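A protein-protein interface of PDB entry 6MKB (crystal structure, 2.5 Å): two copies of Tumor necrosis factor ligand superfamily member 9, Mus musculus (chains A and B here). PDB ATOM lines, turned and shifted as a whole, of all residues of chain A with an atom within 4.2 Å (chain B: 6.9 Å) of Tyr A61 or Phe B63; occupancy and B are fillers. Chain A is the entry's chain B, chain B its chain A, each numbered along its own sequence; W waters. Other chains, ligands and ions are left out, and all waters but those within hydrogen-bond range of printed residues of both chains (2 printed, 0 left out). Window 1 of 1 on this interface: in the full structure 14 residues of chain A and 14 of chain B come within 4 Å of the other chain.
N of Tyr B61 lies within hydrogen-bond range of O of Phe B162 (2.8 Å).
N of Ser B158 is in hydrogen-bond range of O of Glu B65, 2.9 Å away.
The backbone NH (N) of Phe B63 lies within hydrogen-bond range of the backbone carbonyl oxygen (O) of Gly B160.
OH of Tyr B61 is in hydrogen-bond range of OG of Ser B120, at 3.3 Å.
N of Tyr A61 sits at hydrogen-bond distance from O of Phe A162 (2.9 Å).
OH of Tyr A61 sits at hydrogen-bond distance from OG of Ser A120 (3.2 Å).
Among the printed residues, pairs that only touch across the chains: Phe A162 with Phe B162, Phe A63 with Tyr B61, Tyr A61 with Phe B63, Phe A162 with Tyr B61, Val A164 with Phe B10, Phe A162 with Phe B10, Tyr A61 with Tyr B61 and Ser A120 with Glu B65.
Of chain B, only Tyr B61 (3.7 Å) and Phe B63 (3.4 Å) come within 4 Å of Tyr A61.
Phe B63 touches just one residue of chain A: Tyr A61.
Of the printed residues of chain A, Tyr B61 touches Tyr A61 (3.7 Å), Phe A63 (3.4 Å) and Phe A162 (3.5 Å).
Of the printed residues of chain B, Phe A162 touches Phe B10 (3.7 Å), Tyr B61 (3.5 Å) and Phe B162 (3.4 Å).
Of the printed residues of chain B, Val A164 touches Phe B10.
Of the printed residues of chain A, Phe B162 touches Phe A162.
Ser B120 touches none of the printed residues of chain A.
Ala B11 touches none of the printed residues of chain A.
The nearest printed residue of chain A that does not touch Phe B63 is Phe A162 (4.9 Å).
The nearest printed residue of chain B that does not touch Phe A162 is Phe B63 (4.9 Å).
Hydrophobic or aromatic side chains of chain A that line the printed part of chain B: Tyr A61, Phe A63, Phe A162 and Val A164.
Tyr A61 touches its own counterpart, Tyr B61.
Tyr A61 touches Phe B63, and with the chains exchanged Phe A63 touches Tyr B61.
Phe A162 touches Tyr B61, but with the chains exchanged Tyr A61 does not touch Phe B162 (6.7 Å).
Phe A162 touches its own counterpart, Phe B162.
Positions printed for both chains: 61, 62, 63, 120, 121, 161 and 162.
Of the 8 pairs that touch across the chains among the printed residues, 4 have their exchanged pair printed and touching as well.
Water W1 bridges the side-chain carboxylate of Glu B65 and the backbone carbonyl oxygen of Ser A120.
Water W2 lies within hydrogen-bond range of N of Ser A120 (3.0 Å), OG of Ser B118 (3.2 Å) and OE1 of Glu B65 (3.4 Å).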
ATOM      1  N   TYR A  60      -6.686 -10.920   0.103  1.00  0.00           N
ATOM      2  CA  TYR A  60      -7.679 -11.686   0.843  1.00  0.00           C
ATOM      3  C   TYR A  60      -7.582 -11.400   2.323  1.00  0.00           C
ATOM      4  O   TYR A  60      -6.480 -11.287   2.866  1.00  0.00           O
ATOM      5  CB  TYR A  60      -7.498 -13.213   0.622  1.00  0.00           C
ATOM      6  CG  TYR A  60      -7.943 -13.727  -0.730  1.00  0.00           C
ATOM      7  CD1 TYR A  60      -7.121 -13.602  -1.851  1.00  0.00           C
ATOM      8  CD2 TYR A  60      -9.168 -14.372  -0.885  1.00  0.00           C
ATOM      9  CE1 TYR A  60      -7.523 -14.075  -3.101  1.00  0.00           C
ATOM     10  CE2 TYR A  60      -9.575 -14.860  -2.127  1.00  0.00           C
ATOM     11  CZ  TYR A  60      -8.757 -14.693  -3.238  1.00  0.00           C
ATOM     12  OH  TYR A  60      -9.156 -15.159  -4.472  1.00  0.00           O
ATOM     13  N   TYR A  61      -8.740 -11.314   2.981  1.00  0.00           N
ATOM     14  CA  TYR A  61      -8.817 -11.213   4.420  1.00  0.00           C
ATOM     15  C   TYR A  61      -8.881 -12.652   4.889  1.00  0.00           C
ATOM     16  O   TYR A  61      -9.860 -13.338   4.587  1.00  0.00           O
ATOM     17  CB  TYR A  61     -10.039 -10.396   4.823  1.00  0.00           C
ATOM     18  CG  TYR A  61     -10.281 -10.276   6.315  1.00  0.00           C
ATOM     19  CD1 TYR A  61     -10.845 -11.326   7.036  1.00  0.00           C
ATOM     20  CD2 TYR A  61     -10.079  -9.072   6.975  1.00  0.00           C
ATOM     21  CE1 TYR A  61     -11.121 -11.204   8.394  1.00  0.00           C
ATOM     22  CE2 TYR A  61     -10.389  -8.928   8.320  1.00  0.00           C
ATOM     23  CZ  TYR A  61     -10.875 -10.007   9.037  1.00  0.00           C
ATOM     24  OH  TYR A  61     -11.163  -9.876  10.381  1.00  0.00           O
ATOM     25  N   VAL A  62      -7.804 -13.160   5.505  1.00  0.00           N
ATOM     26  CA  VAL A  62      -7.758 -14.551   5.956  1.00  0.00           C
ATOM     27  C   VAL A  62      -7.996 -14.547   7.449  1.00  0.00           C
ATOM     28  O   VAL A  62      -7.473 -13.672   8.151  1.00  0.00           O
ATOM     29  CB  VAL A  62      -6.433 -15.248   5.562  1.00  0.00           C
ATOM     30  CG1 VAL A  62      -6.535 -16.758   5.767  1.00  0.00           C
ATOM     31  CG2 VAL A  62      -6.052 -14.932   4.123  1.00  0.00           C
ATOM     32  N   PHE A  63      -8.838 -15.474   7.936  1.00  0.00           N
ATOM     33  CA  PHE A  63      -9.178 -15.533   9.355  1.00  0.00           C
ATOM     34  C   PHE A  63      -9.101 -16.955   9.883  1.00  0.00           C
ATOM     35  O   PHE A  63      -9.325 -17.927   9.158  1.00  0.00           O
ATOM     36  CB  PHE A  63     -10.566 -14.915   9.633  1.00  0.00           C
ATOM     37  CG  PHE A  63     -11.742 -15.587   8.960  1.00  0.00           C
ATOM     38  CD1 PHE A  63     -12.408 -16.651   9.575  1.00  0.00           C
ATOM     39  CD2 PHE A  63     -12.217 -15.132   7.733  1.00  0.00           C
ATOM     40  CE1 PHE A  63     -13.482 -17.291   8.941  1.00  0.00           C
ATOM     41  CE2 PHE A  63     -13.309 -15.756   7.115  1.00  0.00           C
ATOM     42  CZ  PHE A  63     -13.935 -16.825   7.723  1.00  0.00           C
ATOM     43  N   SER A 120      -6.710 -12.582  12.340  1.00  0.00           N
ATOM     44  CA  SER A 120      -6.914 -12.217  10.933  1.00  0.00           C
ATOM     45  C   SER A 120      -5.704 -11.519  10.378  1.00  0.00           C
ATOM     46  O   SER A 120      -4.932 -10.913  11.123  1.00  0.00           O
ATOM     47  CB  SER A 120      -8.164 -11.359  10.724  1.00  0.00           C
ATOM     48  OG  SER A 120      -8.095 -10.113  11.397  1.00  0.00           O
ATOM     49  N   GLN A 121      -5.535 -11.623   9.054  1.00  0.00           N
ATOM     50  CA  GLN A 121      -4.487 -10.945   8.323  1.00  0.00           C
ATOM     51  C   GLN A 121      -4.919 -10.725   6.883  1.00  0.00           C
ATOM     52  O   GLN A 121      -5.508 -11.626   6.270  1.00  0.00           O
ATOM     53  CB  GLN A 121      -3.168 -11.734   8.376  1.00  0.00           C
ATOM     54  CG  GLN A 121      -1.945 -10.829   8.221  1.00  0.00           C
ATOM     55  CD  GLN A 121      -1.070 -10.925   9.442  1.00  0.00           C
ATOM     56  OE1 GLN A 121      -1.376 -10.356  10.509  1.00  0.00           O
ATOM     57  NE2 GLN A 121       0.004 -11.680   9.334  1.00  0.00           N
ATOM     58  N   LEU A 122      -4.595  -9.541   6.334  1.00  0.00           N
ATOM     59  CA  LEU A 122      -4.835  -9.237   4.940  1.00  0.00           C
ATOM     60  C   LEU A 122      -3.601  -9.715   4.189  1.00  0.00           C
ATOM     61  O   LEU A 122      -2.489  -9.285   4.500  1.00  0.00           O
ATOM     62  CB  LEU A 122      -5.113  -7.741   4.751  1.00  0.00           C
ATOM     63  CG  LEU A 122      -6.521  -7.248   5.130  1.00  0.00           C
ATOM     64  CD1 LEU A 122      -6.513  -5.744   5.405  1.00  0.00           C
ATOM     65  CD2 LEU A 122      -7.557  -7.585   4.038  1.00  0.00           C
ATOM     66  N   LEU A 161     -11.545 -17.188   4.450  1.00  0.00           N
ATOM     67  CA  LEU A 161     -11.031 -16.000   3.763  1.00  0.00           C
ATOM     68  C   LEU A 161     -12.089 -15.407   2.880  1.00  0.00           C
ATOM     69  O   LEU A 161     -13.138 -16.023   2.645  1.00  0.00           O
ATOM     70  CB  LEU A 161      -9.735 -16.250   2.921  1.00  0.00           C
ATOM     71  CG  LEU A 161      -9.544 -17.571   2.120  1.00  0.00           C
ATOM     72  CD1 LEU A 161     -10.634 -17.818   1.141  1.00  0.00           C
ATOM     73  CD2 LEU A 161      -8.288 -17.527   1.341  1.00  0.00           C
ATOM     74  N   PHE A 162     -11.821 -14.186   2.420  1.00  0.00           N
ATOM     75  CA  PHE A 162     -12.649 -13.481   1.476  1.00  0.00           C
ATOM     76  C   PHE A 162     -11.818 -12.531   0.635  1.00  0.00           C
ATOM     77  O   PHE A 162     -10.889 -11.919   1.140  1.00  0.00           O
ATOM     78  CB  PHE A 162     -13.827 -12.758   2.124  1.00  0.00           C
ATOM     79  CG  PHE A 162     -13.667 -11.946   3.372  1.00  0.00           C
ATOM     80  CD1 PHE A 162     -13.333 -10.599   3.302  1.00  0.00           C
ATOM     81  CD2 PHE A 162     -14.047 -12.467   4.616  1.00  0.00           C
ATOM     82  CE1 PHE A 162     -13.324  -9.802   4.469  1.00  0.00           C
ATOM     83  CE2 PHE A 162     -14.033 -11.673   5.776  1.00  0.00           C
ATOM     84  CZ  PHE A 162     -13.696 -10.344   5.693  1.00  0.00           C
ATOM     85  N   VAL A 164     -10.984  -9.251  -0.968  1.00  0.00           N
ATOM     86  CA  VAL A 164     -11.159  -7.835  -0.632  1.00  0.00           C
ATOM     87  C   VAL A 164     -10.819  -6.956  -1.851  1.00  0.00           C
ATOM     88  O   VAL A 164     -11.492  -5.963  -2.120  1.00  0.00           O
ATOM     89  CB  VAL A 164     -10.260  -7.522   0.606  1.00  0.00           C
ATOM     90  CG1 VAL A 164      -9.963  -6.049   0.763  1.00  0.00           C
ATOM     91  CG2 VAL A 164     -10.865  -8.094   1.882  1.00  0.00           C
ATOM     92  N   PHE B  10     -16.379  -3.816   1.244  1.00  0.00           N
ATOM     93  CA  PHE B  10     -15.479  -4.012   2.380  1.00  0.00           C
ATOM     94  C   PHE B  10     -15.068  -2.681   3.010  1.00  0.00           C
ATOM     95  O   PHE B  10     -14.908  -1.688   2.308  1.00  0.00           O
ATOM     96  CB  PHE B  10     -14.215  -4.792   1.920  1.00  0.00           C
ATOM     97  CG  PHE B  10     -13.141  -5.032   2.965  1.00  0.00           C
ATOM     98  CD1 PHE B  10     -13.272  -6.056   3.900  1.00  0.00           C
ATOM     99  CD2 PHE B  10     -11.996  -4.244   3.005  1.00  0.00           C
ATOM    100  CE1 PHE B  10     -12.284  -6.277   4.865  1.00  0.00           C
ATOM    101  CE2 PHE B  10     -11.007  -4.464   3.970  1.00  0.00           C
ATOM    102  CZ  PHE B  10     -11.152  -5.484   4.890  1.00  0.00           C
ATOM    103  N   ALA B  11     -14.845  -2.686   4.329  1.00  0.00           N
ATOM    104  CA  ALA B  11     -14.371  -1.536   5.087  1.00  0.00           C
ATOM    105  C   ALA B  11     -13.492  -1.996   6.219  1.00  0.00           C
ATOM    106  O   ALA B  11     -13.801  -3.012   6.854  1.00  0.00           O
ATOM    107  CB  ALA B  11     -15.550  -0.742   5.649  1.00  0.00           C
ATOM    108  N   LYS B  12     -12.409  -1.241   6.495  1.00  0.00           N
ATOM    109  CA  LYS B  12     -11.535  -1.474   7.641  1.00  0.00           C
ATOM    110  C   LYS B  12     -11.099  -0.124   8.172  1.00  0.00           C
ATOM    111  O   LYS B  12     -10.209   0.518   7.612  1.00  0.00           O
ATOM    112  CB  LYS B  12     -10.338  -2.390   7.330  1.00  0.00           C
ATOM    113  CG  LYS B  12      -9.611  -2.829   8.610  1.00  0.00           C
ATOM    114  CD  LYS B  12      -8.321  -3.601   8.343  1.00  0.00           C
ATOM    115  CE  LYS B  12      -7.508  -3.589   9.617  1.00  0.00           C
ATOM    116  NZ  LYS B  12      -6.267  -4.392   9.536  1.00  0.00           N
ATOM    117  N   LEU B  13     -11.790   0.336   9.219  1.00  0.00           N
ATOM    118  CA  LEU B  13     -11.566   1.620   9.878  1.00  0.00           C
ATOM    119  C   LEU B  13     -10.572   1.437  10.980  1.00  0.00           C
ATOM    120  O   LEU B  13     -10.501   0.358  11.561  1.00  0.00           O
ATOM    121  CB  LEU B  13     -12.886   2.191  10.439  1.00  0.00           C
ATOM    122  CG  LEU B  13     -14.086   2.268   9.482  1.00  0.00           C
ATOM    123  CD1 LEU B  13     -15.291   2.836  10.194  1.00  0.00           C
ATOM    124  CD2 LEU B  13     -13.768   3.085   8.233  1.00  0.00           C
ATOM    125  N   TYR B  61     -19.979 -10.036   7.245  1.00  0.00           N
ATOM    126  CA  TYR B  61     -18.995 -10.540   8.193  1.00  0.00           C
ATOM    127  C   TYR B  61     -18.472  -9.292   8.893  1.00  0.00           C
ATOM    128  O   TYR B  61     -17.802  -8.476   8.253  1.00  0.00           O
ATOM    129  CB  TYR B  61     -17.886 -11.331   7.455  1.00  0.00           C
ATOM    130  CG  TYR B  61     -16.746 -11.814   8.329  1.00  0.00           C
ATOM    131  CD1 TYR B  61     -15.745 -10.940   8.754  1.00  0.00           C
ATOM    132  CD2 TYR B  61     -16.614 -13.163   8.650  1.00  0.00           C
ATOM    133  CE1 TYR B  61     -14.658 -11.392   9.494  1.00  0.00           C
ATOM    134  CE2 TYR B  61     -15.533 -13.622   9.399  1.00  0.00           C
ATOM    135  CZ  TYR B  61     -14.558 -12.730   9.820  1.00  0.00           C
ATOM    136  OH  TYR B  61     -13.501 -13.150  10.586  1.00  0.00           O
ATOM    137  N   VAL B  62     -18.860  -9.086  10.159  1.00  0.00           N
ATOM    138  CA  VAL B  62     -18.458  -7.895  10.901  1.00  0.00           C
ATOM    139  C   VAL B  62     -17.318  -8.280  11.819  1.00  0.00           C
ATOM    140  O   VAL B  62     -17.349  -9.364  12.404  1.00  0.00           O
ATOM    141  CB  VAL B  62     -19.649  -7.265  11.664  1.00  0.00           C
ATOM    142  CG1 VAL B  62     -19.278  -5.875  12.204  1.00  0.00           C
ATOM    143  CG2 VAL B  62     -20.901  -7.190  10.772  1.00  0.00           C
ATOM    144  N   PHE B  63     -16.280  -7.426  11.898  1.00  0.00           N
ATOM    145  CA  PHE B  63     -15.107  -7.729  12.705  1.00  0.00           C
ATOM    146  C   PHE B  63     -14.675  -6.524  13.534  1.00  0.00           C
ATOM    147  O   PHE B  63     -14.886  -5.371  13.147  1.00  0.00           O
ATOM    148  CB  PHE B  63     -13.930  -8.256  11.843  1.00  0.00           C
ATOM    149  CG  PHE B  63     -13.387  -7.308  10.798  1.00  0.00           C
ATOM    150  CD1 PHE B  63     -12.402  -6.356  11.129  1.00  0.00           C
ATOM    151  CD2 PHE B  63     -13.871  -7.334   9.493  1.00  0.00           C
ATOM    152  CE1 PHE B  63     -11.924  -5.455  10.173  1.00  0.00           C
ATOM    153  CE2 PHE B  63     -13.393  -6.423   8.538  1.00  0.00           C
ATOM    154  CZ  PHE B  63     -12.401  -5.514   8.876  1.00  0.00           C
ATOM    155  N   LEU B  64     -14.088  -6.838  14.705  1.00  0.00           N
ATOM    156  CA  LEU B  64     -13.507  -5.952  15.694  1.00  0.00           C
ATOM    157  C   LEU B  64     -12.169  -6.496  16.099  1.00  0.00           C
ATOM    158  O   LEU B  64     -12.036  -7.702  16.321  1.00  0.00           O
ATOM    159  CB  LEU B  64     -14.391  -5.835  16.935  1.00  0.00           C
ATOM    160  CG  LEU B  64     -15.753  -5.172  16.815  1.00  0.00           C
ATOM    161  CD1 LEU B  64     -16.583  -5.408  18.103  1.00  0.00           C
ATOM    162  CD2 LEU B  64     -15.613  -3.666  16.543  1.00  0.00           C
ATOM    163  N   GLU B  65     -11.181  -5.631  16.208  1.00  0.00           N
ATOM    164  CA  GLU B  65      -9.857  -6.030  16.649  1.00  0.00           C
ATOM    165  C   GLU B  65      -9.323  -4.988  17.625  1.00  0.00           C
ATOM    166  O   GLU B  65      -9.069  -3.851  17.235  1.00  0.00           O
ATOM    167  CB  GLU B  65      -8.902  -6.227  15.463  1.00  0.00           C
ATOM    168  CG  GLU B  65      -7.550  -6.718  15.933  1.00  0.00           C
ATOM    169  CD  GLU B  65      -6.624  -7.188  14.837  1.00  0.00           C
ATOM    170  OE1 GLU B  65      -5.477  -7.556  15.169  1.00  0.00           O
ATOM    171  OE2 GLU B  65      -7.031  -7.182  13.653  1.00  0.00           O
ATOM    172  N   LEU B  87     -20.269  -3.643  19.900  1.00  0.00           N
ATOM    173  CA  LEU B  87     -20.873  -3.285  18.614  1.00  0.00           C
ATOM    174  C   LEU B  87     -22.298  -2.794  18.867  1.00  0.00           C
ATOM    175  O   LEU B  87     -23.112  -3.548  19.388  1.00  0.00           O
ATOM    176  CB  LEU B  87     -20.846  -4.475  17.627  1.00  0.00           C
ATOM    177  CG  LEU B  87     -21.388  -4.192  16.213  1.00  0.00           C
ATOM    178  CD1 LEU B  87     -20.466  -3.238  15.436  1.00  0.00           C
ATOM    179  CD2 LEU B  87     -21.584  -5.480  15.433  1.00  0.00           C
ATOM    180  N   SER B 118      -9.031 -10.295  18.513  1.00  0.00           N
ATOM    181  CA  SER B 118      -9.963 -10.154  17.400  1.00  0.00           C
ATOM    182  C   SER B 118     -11.296 -10.815  17.731  1.00  0.00           C
ATOM    183  O   SER B 118     -11.343 -11.752  18.525  1.00  0.00           O
ATOM    184  CB  SER B 118      -9.376 -10.749  16.128  1.00  0.00           C
ATOM    185  OG  SER B 118      -8.162 -10.113  15.773  1.00  0.00           O
ATOM    186  N   TRP B 119     -12.372 -10.320  17.104  1.00  0.00           N
ATOM    187  CA  TRP B 119     -13.742 -10.793  17.211  1.00  0.00           C
ATOM    188  C   TRP B 119     -14.426 -10.720  15.844  1.00  0.00           C
ATOM    189  O   TRP B 119     -14.146  -9.813  15.068  1.00  0.00           O
ATOM    190  CB  TRP B 119     -14.486  -9.928  18.233  1.00  0.00           C
ATOM    191  CG  TRP B 119     -15.963 -10.162  18.375  1.00  0.00           C
ATOM    192  CD1 TRP B 119     -16.583 -10.912  19.327  1.00  0.00           C
ATOM    193  CD2 TRP B 119     -17.010  -9.544  17.602  1.00  0.00           C
ATOM    194  NE1 TRP B 119     -17.954 -10.818  19.187  1.00  0.00           N
ATOM    195  CE2 TRP B 119     -18.243  -9.988  18.136  1.00  0.00           C
ATOM    196  CE3 TRP B 119     -17.025  -8.669  16.494  1.00  0.00           C
ATOM    197  CZ2 TRP B 119     -19.478  -9.605  17.593  1.00  0.00           C
ATOM    198  CZ3 TRP B 119     -18.248  -8.266  15.973  1.00  0.00           C
ATOM    199  CH2 TRP B 119     -19.457  -8.742  16.513  1.00  0.00           C
ATOM    200  N   SER B 120     -15.350 -11.631  15.568  1.00  0.00           N
ATOM    201  CA  SER B 120     -16.137 -11.574  14.342  1.00  0.00           C
ATOM    202  C   SER B 120     -17.479 -12.246  14.521  1.00  0.00           C
ATOM    203  O   SER B 120     -17.626 -13.121  15.381  1.00  0.00           O
ATOM    204  CB  SER B 120     -15.408 -12.206  13.160  1.00  0.00           C
ATOM    205  OG  SER B 120     -15.179 -13.596  13.336  1.00  0.00           O
ATOM    206  N   GLN B 121     -18.453 -11.818  13.703  1.00  0.00           N
ATOM    207  CA  GLN B 121     -19.787 -12.394  13.662  1.00  0.00           C
ATOM    208  C   GLN B 121     -20.434 -12.109  12.308  1.00  0.00           C
ATOM    209  O   GLN B 121     -20.282 -11.019  11.751  1.00  0.00           O
ATOM    210  CB  GLN B 121     -20.666 -11.885  14.815  1.00  0.00           C
ATOM    211  CG  GLN B 121     -21.723 -12.908  15.261  1.00  0.00           C
ATOM    212  CD  GLN B 121     -22.175 -12.769  16.702  1.00  0.00           C
ATOM    213  OE1 GLN B 121     -23.349 -12.959  17.021  1.00  0.00           O
ATOM    214  NE2 GLN B 121     -21.267 -12.451  17.616  1.00  0.00           N
ATOM    215  N   VAL B 133     -19.225   1.751  17.631  1.00  0.00           N
ATOM    216  CA  VAL B 133     -18.489   0.896  18.555  1.00  0.00           C
ATOM    217  C   VAL B 133     -18.224   1.651  19.851  1.00  0.00           C
ATOM    218  O   VAL B 133     -17.621   2.724  19.838  1.00  0.00           O
ATOM    219  CB  VAL B 133     -17.173   0.349  17.933  1.00  0.00           C
ATOM    220  CG1 VAL B 133     -16.439  -0.580  18.903  1.00  0.00           C
ATOM    221  CG2 VAL B 133     -17.441  -0.371  16.617  1.00  0.00           C
ATOM    222  N   SER B 158      -9.105  -1.752  15.164  1.00  0.00           N
ATOM    223  CA  SER B 158      -9.828  -1.679  13.908  1.00  0.00           C
ATOM    224  C   SER B 158     -11.232  -2.231  14.021  1.00  0.00           C
ATOM    225  O   SER B 158     -11.574  -2.991  14.932  1.00  0.00           O
ATOM    226  CB  SER B 158      -9.070  -2.402  12.798  1.00  0.00           C
ATOM    227  OG  SER B 158      -8.968  -3.777  13.105  1.00  0.00           O
ATOM    228  N   PHE B 159     -12.027  -1.851  13.038  1.00  0.00           N
ATOM    229  CA  PHE B 159     -13.402  -2.197  12.918  1.00  0.00           C
ATOM    230  C   PHE B 159     -13.772  -2.133  11.473  1.00  0.00           C
ATOM    231  O   PHE B 159     -13.456  -1.159  10.782  1.00  0.00           O
ATOM    232  CB  PHE B 159     -14.245  -1.223  13.762  1.00  0.00           C
ATOM    233  CG  PHE B 159     -15.682  -1.052  13.357  1.00  0.00           C
ATOM    234  CD1 PHE B 159     -16.555  -2.138  13.342  1.00  0.00           C
ATOM    235  CD2 PHE B 159     -16.181   0.200  13.037  1.00  0.00           C
ATOM    236  CE1 PHE B 159     -17.882  -1.978  12.969  1.00  0.00           C
ATOM    237  CE2 PHE B 159     -17.525   0.366  12.702  1.00  0.00           C
ATOM    238  CZ  PHE B 159     -18.363  -0.726  12.669  1.00  0.00           C
ATOM    239  N   GLY B 160     -14.502  -3.143  11.043  1.00  0.00           N
ATOM    240  CA  GLY B 160     -14.993  -3.190   9.683  1.00  0.00           C
ATOM    241  C   GLY B 160     -15.976  -4.300   9.426  1.00  0.00           C
ATOM    242  O   GLY B 160     -16.491  -4.930  10.353  1.00  0.00           O
ATOM    243  N   LEU B 161     -16.206  -4.552   8.145  1.00  0.00           N
ATOM    244  CA  LEU B 161     -17.127  -5.573   7.668  1.00  0.00           C
ATOM    245  C   LEU B 161     -16.918  -5.832   6.187  1.00  0.00           C
ATOM    246  O   LEU B 161     -16.223  -5.070   5.524  1.00  0.00           O
ATOM    247  CB  LEU B 161     -18.621  -5.238   7.962  1.00  0.00           C
ATOM    248  CG  LEU B 161     -19.108  -3.780   7.885  1.00  0.00           C
ATOM    249  CD1 LEU B 161     -18.901  -3.171   6.492  1.00  0.00           C
ATOM    250  CD2 LEU B 161     -20.572  -3.675   8.315  1.00  0.00           C
ATOM    251  N   PHE B 162     -17.523  -6.916   5.688  1.00  0.00           N
ATOM    252  CA  PHE B 162     -17.517  -7.332   4.294  1.00  0.00           C
ATOM    253  C   PHE B 162     -18.868  -7.952   3.982  1.00  0.00           C
ATOM    254  O   PHE B 162     -19.381  -8.689   4.818  1.00  0.00           O
ATOM    255  CB  PHE B 162     -16.367  -8.321   4.056  1.00  0.00           C
ATOM    256  CG  PHE B 162     -16.366  -9.115   2.768  1.00  0.00           C
ATOM    257  CD1 PHE B 162     -16.906 -10.401   2.723  1.00  0.00           C
ATOM    258  CD2 PHE B 162     -15.690  -8.644   1.640  1.00  0.00           C
ATOM    259  CE1 PHE B 162     -16.865 -11.158   1.541  1.00  0.00           C
ATOM    260  CE2 PHE B 162     -15.627  -9.409   0.472  1.00  0.00           C
ATOM    261  CZ  PHE B 162     -16.213 -10.666   0.432  1.00  0.00           C
HETATM  262  O   HOH W   1      -5.302  -8.467  12.212  1.00  0.00           O
HETATM  263  O   HOH W   2      -5.382 -10.922  14.468  1.00  0.00           O
